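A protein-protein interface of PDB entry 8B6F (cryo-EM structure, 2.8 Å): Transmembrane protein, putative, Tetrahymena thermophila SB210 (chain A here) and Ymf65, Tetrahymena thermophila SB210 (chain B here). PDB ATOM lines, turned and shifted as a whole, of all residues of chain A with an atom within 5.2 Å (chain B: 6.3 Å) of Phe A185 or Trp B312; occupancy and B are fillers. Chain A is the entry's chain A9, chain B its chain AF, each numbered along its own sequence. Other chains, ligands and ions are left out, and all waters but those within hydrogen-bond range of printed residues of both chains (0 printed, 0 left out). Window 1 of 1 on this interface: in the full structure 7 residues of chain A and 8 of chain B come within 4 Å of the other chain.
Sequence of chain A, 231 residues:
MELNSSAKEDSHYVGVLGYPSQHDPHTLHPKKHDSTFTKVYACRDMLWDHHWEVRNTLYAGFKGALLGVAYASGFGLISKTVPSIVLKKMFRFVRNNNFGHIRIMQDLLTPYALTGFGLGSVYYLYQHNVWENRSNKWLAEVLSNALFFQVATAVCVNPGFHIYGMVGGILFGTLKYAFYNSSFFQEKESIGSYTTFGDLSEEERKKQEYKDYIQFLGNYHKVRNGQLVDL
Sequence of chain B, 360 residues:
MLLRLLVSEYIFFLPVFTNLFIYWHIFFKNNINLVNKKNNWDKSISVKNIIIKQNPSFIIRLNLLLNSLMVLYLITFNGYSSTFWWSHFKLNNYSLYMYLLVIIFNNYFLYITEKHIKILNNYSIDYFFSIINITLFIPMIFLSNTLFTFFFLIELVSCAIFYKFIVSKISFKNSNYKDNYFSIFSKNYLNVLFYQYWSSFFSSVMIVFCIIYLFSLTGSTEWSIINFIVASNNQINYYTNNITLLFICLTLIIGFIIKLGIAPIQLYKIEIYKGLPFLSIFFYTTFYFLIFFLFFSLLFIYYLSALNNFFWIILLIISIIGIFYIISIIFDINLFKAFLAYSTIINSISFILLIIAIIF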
ATOM      1  N   MET A   1     -22.280 -21.208  21.854  1.00  0.00           N
ATOM      2  CA  MET A   1     -21.455 -22.068  20.960  1.00  0.00           C
ATOM      3  C   MET A   1     -20.644 -23.080  21.762  1.00  0.00           C
ATOM      4  O   MET A   1     -19.898 -22.709  22.667  1.00  0.00           O
ATOM      5  CB  MET A   1     -20.517 -21.211  20.110  1.00  0.00           C
ATOM      6  CG  MET A   1     -21.236 -20.168  19.271  1.00  0.00           C
ATOM      7  SD  MET A   1     -20.135 -19.259  18.171  1.00  0.00           S
ATOM      8  CE  MET A   1     -19.554 -20.569  17.099  1.00  0.00           C
ATOM      9  N   LEU A   3     -18.240 -26.876  21.528  1.00  0.00           N
ATOM     10  CA  LEU A   3     -17.442 -27.790  20.723  1.00  0.00           C
ATOM     11  C   LEU A   3     -17.522 -29.182  21.334  1.00  0.00           C
ATOM     12  O   LEU A   3     -17.220 -29.358  22.518  1.00  0.00           O
ATOM     13  CB  LEU A   3     -15.983 -27.333  20.646  1.00  0.00           C
ATOM     14  CG  LEU A   3     -15.675 -25.986  19.981  1.00  0.00           C
ATOM     15  CD1 LEU A   3     -16.152 -24.802  20.812  1.00  0.00           C
ATOM     16  CD2 LEU A   3     -14.188 -25.865  19.701  1.00  0.00           C
ATOM     17  N   PHE A 179     -10.755 -26.691  25.383  1.00  0.00           N
ATOM     18  CA  PHE A 179     -12.027 -26.190  24.882  1.00  0.00           C
ATOM     19  C   PHE A 179     -12.787 -27.173  23.999  1.00  0.00           C
ATOM     20  O   PHE A 179     -13.840 -26.807  23.467  1.00  0.00           O
ATOM     21  CB  PHE A 179     -11.808 -24.881  24.112  1.00  0.00           C
ATOM     22  CG  PHE A 179     -11.315 -23.756  24.972  1.00  0.00           C
ATOM     23  CD1 PHE A 179     -12.109 -23.241  25.981  1.00  0.00           C
ATOM     24  CD2 PHE A 179     -10.066 -23.205  24.763  1.00  0.00           C
ATOM     25  CE1 PHE A 179     -11.659 -22.206  26.774  1.00  0.00           C
ATOM     26  CE2 PHE A 179      -9.611 -22.171  25.552  1.00  0.00           C
ATOM     27  CZ  PHE A 179     -10.408 -21.668  26.557  1.00  0.00           C
ATOM     28  N   SER A 183     -15.406 -28.506  29.145  1.00  0.00           N
ATOM     29  CA  SER A 183     -16.460 -27.503  29.041  1.00  0.00           C
ATOM     30  C   SER A 183     -16.117 -26.348  29.979  1.00  0.00           C
ATOM     31  O   SER A 183     -16.498 -26.346  31.150  1.00  0.00           O
ATOM     32  CB  SER A 183     -17.812 -28.121  29.378  1.00  0.00           C
ATOM     33  OG  SER A 183     -18.847 -27.161  29.287  1.00  0.00           O
ATOM     34  N   PHE A 184     -15.394 -25.361  29.452  1.00  0.00           N
ATOM     35  CA  PHE A 184     -15.060 -24.152  30.196  1.00  0.00           C
ATOM     36  C   PHE A 184     -16.004 -22.997  29.904  1.00  0.00           C
ATOM     37  O   PHE A 184     -16.430 -22.303  30.831  1.00  0.00           O
ATOM     38  CB  PHE A 184     -13.623 -23.718  29.894  1.00  0.00           C
ATOM     39  CG  PHE A 184     -12.596 -24.388  30.756  1.00  0.00           C
ATOM     40  CD1 PHE A 184     -12.473 -24.047  32.093  1.00  0.00           C
ATOM     41  CD2 PHE A 184     -11.749 -25.346  30.232  1.00  0.00           C
ATOM     42  CE1 PHE A 184     -11.529 -24.657  32.894  1.00  0.00           C
ATOM     43  CE2 PHE A 184     -10.803 -25.962  31.025  1.00  0.00           C
ATOM     44  CZ  PHE A 184     -10.692 -25.617  32.360  1.00  0.00           C
ATOM     45  N   PHE A 185     -16.332 -22.765  28.636  1.00  0.00           N
ATOM     46  CA  PHE A 185     -17.326 -21.772  28.252  1.00  0.00           C
ATOM     47  C   PHE A 185     -18.609 -22.414  27.744  1.00  0.00           C
ATOM     48  O   PHE A 185     -19.435 -21.730  27.132  1.00  0.00           O
ATOM     49  CB  PHE A 185     -16.751 -20.832  27.191  1.00  0.00           C
ATOM     50  CG  PHE A 185     -15.642 -19.958  27.697  1.00  0.00           C
ATOM     51  CD1 PHE A 185     -14.333 -20.405  27.693  1.00  0.00           C
ATOM     52  CD2 PHE A 185     -15.909 -18.688  28.176  1.00  0.00           C
ATOM     53  CE1 PHE A 185     -13.312 -19.601  28.157  1.00  0.00           C
ATOM     54  CE2 PHE A 185     -14.893 -17.880  28.642  1.00  0.00           C
ATOM     55  CZ  PHE A 185     -13.592 -18.337  28.632  1.00  0.00           C
ATOM     56  N   GLN A 186     -18.792 -23.711  27.984  1.00  0.00           N
ATOM     57  CA  GLN A 186     -19.951 -24.456  27.511  1.00  0.00           C
ATOM     58  C   GLN A 186     -20.699 -25.111  28.666  1.00  0.00           C
ATOM     59  O   GLN A 186     -21.290 -26.179  28.503  1.00  0.00           O
ATOM     60  CB  GLN A 186     -19.535 -25.516  26.490  1.00  0.00           C
ATOM     61  CG  GLN A 186     -18.622 -25.019  25.380  1.00  0.00           C
ATOM     62  CD  GLN A 186     -17.176 -24.894  25.813  1.00  0.00           C
ATOM     63  OE1 GLN A 186     -16.883 -24.701  26.992  1.00  0.00           O
ATOM     64  NE2 GLN A 186     -16.262 -25.016  24.860  1.00  0.00           N
ATOM     65  N   GLU A 187     -20.671 -24.490  29.843  1.00  0.00           N
ATOM     66  CA  GLU A 187     -21.275 -25.103  31.019  1.00  0.00           C
ATOM     67  C   GLU A 187     -22.763 -25.337  30.804  1.00  0.00           C
ATOM     68  O   GLU A 187     -23.488 -24.446  30.352  1.00  0.00           O
ATOM     69  CB  GLU A 187     -21.063 -24.222  32.250  1.00  0.00           C
ATOM     70  CG  GLU A 187     -19.704 -24.380  32.906  1.00  0.00           C
ATOM     71  CD  GLU A 187     -18.579 -23.833  32.058  1.00  0.00           C
ATOM     72  OE1 GLU A 187     -18.869 -23.164  31.046  1.00  0.00           O
ATOM     73  OE2 GLU A 187     -17.404 -24.071  32.407  1.00  0.00           O
ATOM     74  N   LEU B 307     -24.313 -11.553  25.567  1.00  0.00           N
ATOM     75  CA  LEU B 307     -23.863 -12.230  24.359  1.00  0.00           C
ATOM     76  C   LEU B 307     -22.502 -12.891  24.531  1.00  0.00           C
ATOM     77  O   LEU B 307     -21.918 -13.343  23.543  1.00  0.00           O
ATOM     78  CB  LEU B 307     -23.813 -11.243  23.192  1.00  0.00           C
ATOM     79  CG  LEU B 307     -25.160 -10.761  22.650  1.00  0.00           C
ATOM     80  CD1 LEU B 307     -24.964  -9.602  21.692  1.00  0.00           C
ATOM     81  CD2 LEU B 307     -25.893 -11.897  21.958  1.00  0.00           C
ATOM     82  N   ASN B 308     -21.989 -12.970  25.760  1.00  0.00           N
ATOM     83  CA  ASN B 308     -20.659 -13.529  25.973  1.00  0.00           C
ATOM     84  C   ASN B 308     -20.571 -14.995  25.572  1.00  0.00           C
ATOM     85  O   ASN B 308     -19.461 -15.506  25.388  1.00  0.00           O
ATOM     86  CB  ASN B 308     -20.248 -13.374  27.436  1.00  0.00           C
ATOM     87  CG  ASN B 308     -19.758 -11.980  27.758  1.00  0.00           C
ATOM     88  OD1 ASN B 308     -19.212 -11.289  26.900  1.00  0.00           O
ATOM     89  ND2 ASN B 308     -19.944 -11.559  29.004  1.00  0.00           N
ATOM     90  N   ASN B 309     -21.703 -15.685  25.439  1.00  0.00           N
ATOM     91  CA  ASN B 309     -21.671 -17.063  24.959  1.00  0.00           C
ATOM     92  C   ASN B 309     -21.185 -17.158  23.520  1.00  0.00           C
ATOM     93  O   ASN B 309     -20.796 -18.245  23.082  1.00  0.00           O
ATOM     94  CB  ASN B 309     -23.055 -17.701  25.090  1.00  0.00           C
ATOM     95  CG  ASN B 309     -24.150 -16.843  24.499  1.00  0.00           C
ATOM     96  OD1 ASN B 309     -23.882 -15.872  23.795  1.00  0.00           O
ATOM     97  ND2 ASN B 309     -25.397 -17.196  24.788  1.00  0.00           N
ATOM     98  N   PHE B 310     -21.201 -16.052  22.776  1.00  0.00           N
ATOM     99  CA  PHE B 310     -20.623 -15.992  21.439  1.00  0.00           C
ATOM    100  C   PHE B 310     -19.291 -15.257  21.398  1.00  0.00           C
ATOM    101  O   PHE B 310     -18.424 -15.617  20.598  1.00  0.00           O
ATOM    102  CB  PHE B 310     -21.589 -15.299  20.473  1.00  0.00           C
ATOM    103  CG  PHE B 310     -22.860 -16.059  20.222  1.00  0.00           C
ATOM    104  CD1 PHE B 310     -22.914 -17.045  19.253  1.00  0.00           C
ATOM    105  CD2 PHE B 310     -24.010 -15.766  20.936  1.00  0.00           C
ATOM    106  CE1 PHE B 310     -24.087 -17.738  19.014  1.00  0.00           C
ATOM    107  CE2 PHE B 310     -25.184 -16.455  20.703  1.00  0.00           C
ATOM    108  CZ  PHE B 310     -25.222 -17.442  19.740  1.00  0.00           C
ATOM    109  N   PHE B 311     -19.108 -14.243  22.247  1.00  0.00           N
ATOM    110  CA  PHE B 311     -17.906 -13.419  22.177  1.00  0.00           C
ATOM    111  C   PHE B 311     -16.656 -14.195  22.563  1.00  0.00           C
ATOM    112  O   PHE B 311     -15.567 -13.889  22.067  1.00  0.00           O
ATOM    113  CB  PHE B 311     -18.043 -12.193  23.086  1.00  0.00           C
ATOM    114  CG  PHE B 311     -19.046 -11.176  22.613  1.00  0.00           C
ATOM    115  CD1 PHE B 311     -19.252 -10.944  21.265  1.00  0.00           C
ATOM    116  CD2 PHE B 311     -19.778 -10.441  23.531  1.00  0.00           C
ATOM    117  CE1 PHE B 311     -20.168 -10.002  20.841  1.00  0.00           C
ATOM    118  CE2 PHE B 311     -20.696  -9.499  23.113  1.00  0.00           C
ATOM    119  CZ  PHE B 311     -20.891  -9.279  21.767  1.00  0.00           C
ATOM    120  N   TRP B 312     -16.783 -15.197  23.433  1.00  0.00           N
ATOM    121  CA  TRP B 312     -15.598 -15.842  23.987  1.00  0.00           C
ATOM    122  C   TRP B 312     -14.777 -16.512  22.890  1.00  0.00           C
ATOM    123  O   TRP B 312     -13.551 -16.373  22.846  1.00  0.00           O
ATOM    124  CB  TRP B 312     -15.999 -16.856  25.060  1.00  0.00           C
ATOM    125  CG  TRP B 312     -16.689 -18.070  24.520  1.00  0.00           C
ATOM    126  CD1 TRP B 312     -18.016 -18.203  24.244  1.00  0.00           C
ATOM    127  CD2 TRP B 312     -16.081 -19.324  24.186  1.00  0.00           C
ATOM    128  NE1 TRP B 312     -18.274 -19.462  23.759  1.00  0.00           N
ATOM    129  CE2 TRP B 312     -17.102 -20.171  23.713  1.00  0.00           C
ATOM    130  CE3 TRP B 312     -14.771 -19.813  24.240  1.00  0.00           C
ATOM    131  CZ2 TRP B 312     -16.857 -21.477  23.298  1.00  0.00           C
ATOM    132  CZ3 TRP B 312     -14.528 -21.112  23.828  1.00  0.00           C
ATOM    133  CH2 TRP B 312     -15.567 -21.930  23.362  1.00  0.00           C
ATOM    134  N   ILE B 313     -15.439 -17.247  21.996  1.00  0.00           N
ATOM    135  CA  ILE B 313     -14.707 -17.982  20.969  1.00  0.00           C
ATOM    136  C   ILE B 313     -14.075 -17.017  19.975  1.00  0.00           C
ATOM    137  O   ILE B 313     -12.931 -17.205  19.549  1.00  0.00           O
ATOM    138  CB  ILE B 313     -15.635 -18.998  20.276  1.00  0.00           C
ATOM    139  CG1 ILE B 313     -14.837 -19.925  19.355  1.00  0.00           C
ATOM    140  CG2 ILE B 313     -16.724 -18.294  19.479  1.00  0.00           C
ATOM    141  CD1 ILE B 313     -13.847 -20.821  20.075  1.00  0.00           C
ATOM    142  N   ILE B 314     -14.802 -15.963  19.599  1.00  0.00           N
ATOM    143  CA  ILE B 314     -14.257 -14.981  18.666  1.00  0.00           C
ATOM    144  C   ILE B 314     -13.034 -14.306  19.270  1.00  0.00           C
ATOM    145  O   ILE B 314     -12.008 -14.132  18.603  1.00  0.00           O
ATOM    146  CB  ILE B 314     -15.334 -13.953  18.274  1.00  0.00           C
ATOM    147  CG1 ILE B 314     -16.554 -14.658  17.675  1.00  0.00           C
ATOM    148  CG2 ILE B 314     -14.772 -12.951  17.276  1.00  0.00           C
ATOM    149  CD1 ILE B 314     -17.748 -13.752  17.468  1.00  0.00           C
ATOM    150  N   LEU B 315     -13.123 -13.913  20.540  1.00  0.00           N
ATOM    151  CA  LEU B 315     -11.986 -13.279  21.193  1.00  0.00           C
ATOM    152  C   LEU B 315     -10.796 -14.224  21.259  1.00  0.00           C
ATOM    153  O   LEU B 315      -9.656 -13.817  21.013  1.00  0.00           O
ATOM    154  CB  LEU B 315     -12.377 -12.817  22.597  1.00  0.00           C
ATOM    155  CG  LEU B 315     -13.347 -11.637  22.685  1.00  0.00           C
ATOM    156  CD1 LEU B 315     -13.736 -11.383  24.130  1.00  0.00           C
ATOM    157  CD2 LEU B 315     -12.740 -10.386  22.068  1.00  0.00           C
ATOM    158  N   LEU B 316     -11.040 -15.493  21.590  1.00  0.00           N
ATOM    159  CA  LEU B 316      -9.944 -16.452  21.677  1.00  0.00           C
ATOM    160  C   LEU B 316      -9.269 -16.633  20.324  1.00  0.00           C
ATOM    161  O   LEU B 316      -8.037 -16.615  20.225  1.00  0.00           O
ATOM    162  CB  LEU B 316     -10.461 -17.790  22.207  1.00  0.00           C
ATOM    163  CG  LEU B 316      -9.400 -18.863  22.466  1.00  0.00           C
ATOM    164  CD1 LEU B 316      -8.422 -18.421  23.544  1.00  0.00           C
ATOM    165  CD2 LEU B 316     -10.057 -20.174  22.848  1.00  0.00           C
ATOM    166  N   ILE B 317     -10.059 -16.797  19.262  1.00  0.00           N
ATOM    167  CA  ILE B 317      -9.484 -16.986  17.933  1.00  0.00           C
ATOM    168  C   ILE B 317      -8.671 -15.761  17.534  1.00  0.00           C
ATOM    169  O   ILE B 317      -7.550 -15.874  17.029  1.00  0.00           O
ATOM    170  CB  ILE B 317     -10.588 -17.294  16.906  1.00  0.00           C
ATOM    171  CG1 ILE B 317     -11.257 -18.631  17.236  1.00  0.00           C
ATOM    172  CG2 ILE B 317     -10.015 -17.329  15.493  1.00  0.00           C
ATOM    173  CD1 ILE B 317     -12.501 -18.918  16.428  1.00  0.00           C
ATOM    174  N   ILE B 356     -10.907 -11.903  28.173  1.00  0.00           N
ATOM    175  CA  ILE B 356     -11.449 -13.254  28.062  1.00  0.00           C
ATOM    176  C   ILE B 356     -11.517 -13.895  29.441  1.00  0.00           C
ATOM    177  O   ILE B 356     -12.527 -14.500  29.817  1.00  0.00           O
ATOM    178  CB  ILE B 356     -10.606 -14.093  27.086  1.00  0.00           C
ATOM    179  CG1 ILE B 356     -10.674 -13.494  25.680  1.00  0.00           C
ATOM    180  CG2 ILE B 356     -11.098 -15.536  27.061  1.00  0.00           C
ATOM    181  CD1 ILE B 356      -9.700 -14.113  24.702  1.00  0.00           C
ATOM    182  N   ALA B 357     -10.435 -13.781  30.210  1.00  0.00           N
ATOM    183  CA  ALA B 357     -10.425 -14.337  31.559  1.00  0.00           C
ATOM    184  C   ALA B 357     -11.537 -13.736  32.410  1.00  0.00           C
ATOM    185  O   ALA B 357     -12.185 -14.445  33.187  1.00  0.00           O
ATOM    186  CB  ALA B 357      -9.064 -14.098  32.213  1.00  0.00           C
ATOM    187  N   ILE B 359     -14.476 -12.322  31.403  1.00  0.00           N
ATOM    188  CA  ILE B 359     -15.810 -12.726  30.977  1.00  0.00           C
ATOM    189  C   ILE B 359     -16.073 -14.201  31.241  1.00  0.00           C
ATOM    190  O   ILE B 359     -17.235 -14.619  31.259  1.00  0.00           O
ATOM    191  CB  ILE B 359     -16.042 -12.405  29.487  1.00  0.00           C
ATOM    192  CG1 ILE B 359     -15.083 -13.209  28.603  1.00  0.00           C
ATOM    193  CG2 ILE B 359     -15.893 -10.909  29.248  1.00  0.00           C
ATOM    194  CD1 ILE B 359     -15.300 -13.019  27.113  1.00  0.00           C
ATOM    195  N   PHE B 360     -15.033 -15.007  31.434  1.00  0.00           N
ATOM    196  CA  PHE B 360     -15.224 -16.406  31.805  1.00  0.00           C
ATOM    197  C   PHE B 360     -16.183 -16.524  32.983  1.00  0.00           C
ATOM    198  O   PHE B 360     -16.332 -15.597  33.776  1.00  0.00           O
ATOM    199  CB  PHE B 360     -13.893 -17.073  32.155  1.00  0.00           C
ATOM    200  CG  PHE B 360     -14.046 -18.461  32.712  1.00  0.00           C
ATOM    201  CD1 PHE B 360     -14.205 -19.544  31.865  1.00  0.00           C
ATOM    202  CD2 PHE B 360     -14.048 -18.681  34.078  1.00  0.00           C
ATOM    203  CE1 PHE B 360     -14.352 -20.821  32.369  1.00  0.00           C
ATOM    204  CE2 PHE B 360     -14.195 -19.957  34.590  1.00  0.00           C
ATOM    205  CZ  PHE B 360     -14.347 -21.029  33.733  1.00  0.00           C
ATOM    206  OXT PHE B 360     -16.830 -17.553  33.169  1.00  0.00           O
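Of the 8 printed residues of chain A, 6 touch a printed residue of chain B. Printed residues of chain A that touch a printed residue of chain B: Met A1, Leu A3, Phe A179, Phe A184, Phe A185 and Gln A186. Hydrophobic or aromatic side chains of chain A that line the printed part of chain B: Met A1, Leu A3, Phe A179, Phe A184 and Phe A185. Among the printed residues, no Asp or Glu carboxylate lies within 4 Å of a Lys or Arg side-chain nitrogen of the other chain.
Among the printed residues, merely in contact across the chains: Phe A184 with Phe B360 (3.0 Å), Met A1 with Trp B312 (3.3 Å), Phe A179 with Leu B316 (3.4 Å), Phe A185 with Trp B312 (3.4 Å), Gln A186 with Trp B312 (3.5 Å), Phe A185 with Phe B360 (3.5 Å), Met A1 with Asn B309 (3.5 Å), Met A1 with Phe B310 (3.5 Å), Met A1 with Ile B313 (3.8 Å), Phe A179 with Trp B312 (3.9 Å) and Leu A3 with Trp B312 (3.9 Å).
The side-chain amide nitrogen (NE2) of Gln A186 sits at hydrogen-bond distance from the backbone carbonyl oxygen (O) of Phe A179, 3.3 Å away. The backbone carbonyl oxygen of Gln A186 is in hydrogen-bond range of the side-chain hydroxyl of Ser A183 (2.7 Å). The backbone NH (N) of Phe A184 is in hydrogen-bond range of the side-chain amide oxygen (OE1) of Gln A186 (3.0 Å). O of Phe A184 lies close to OE2 of Glu A187. The side-chain amide oxygen (OD1) of Asn B309 lies close to the backbone carbonyl oxygen (O) of Leu B307 (3.2 Å). The indole nitrogen (NE1) of Trp B312 is in hydrogen-bond range of the backbone carbonyl oxygen (O) of Asn B309, at 2.9 Å.
Of the printed residues of chain B, Leu A3 touches Trp B312 (3.9 Å). Printed residues of chain B within 4 Å of Phe A184: Phe B360. Glu A187 touches none of the printed residues of chain B. Ile B359 touches none of the printed residues of chain A. The nearest residue of chain B that does not touch Phe A185 is Ile B356 (4.1 Å). The nearest printed residue of chain B that does not touch Phe A179 is Ile B313 (6.1 Å).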
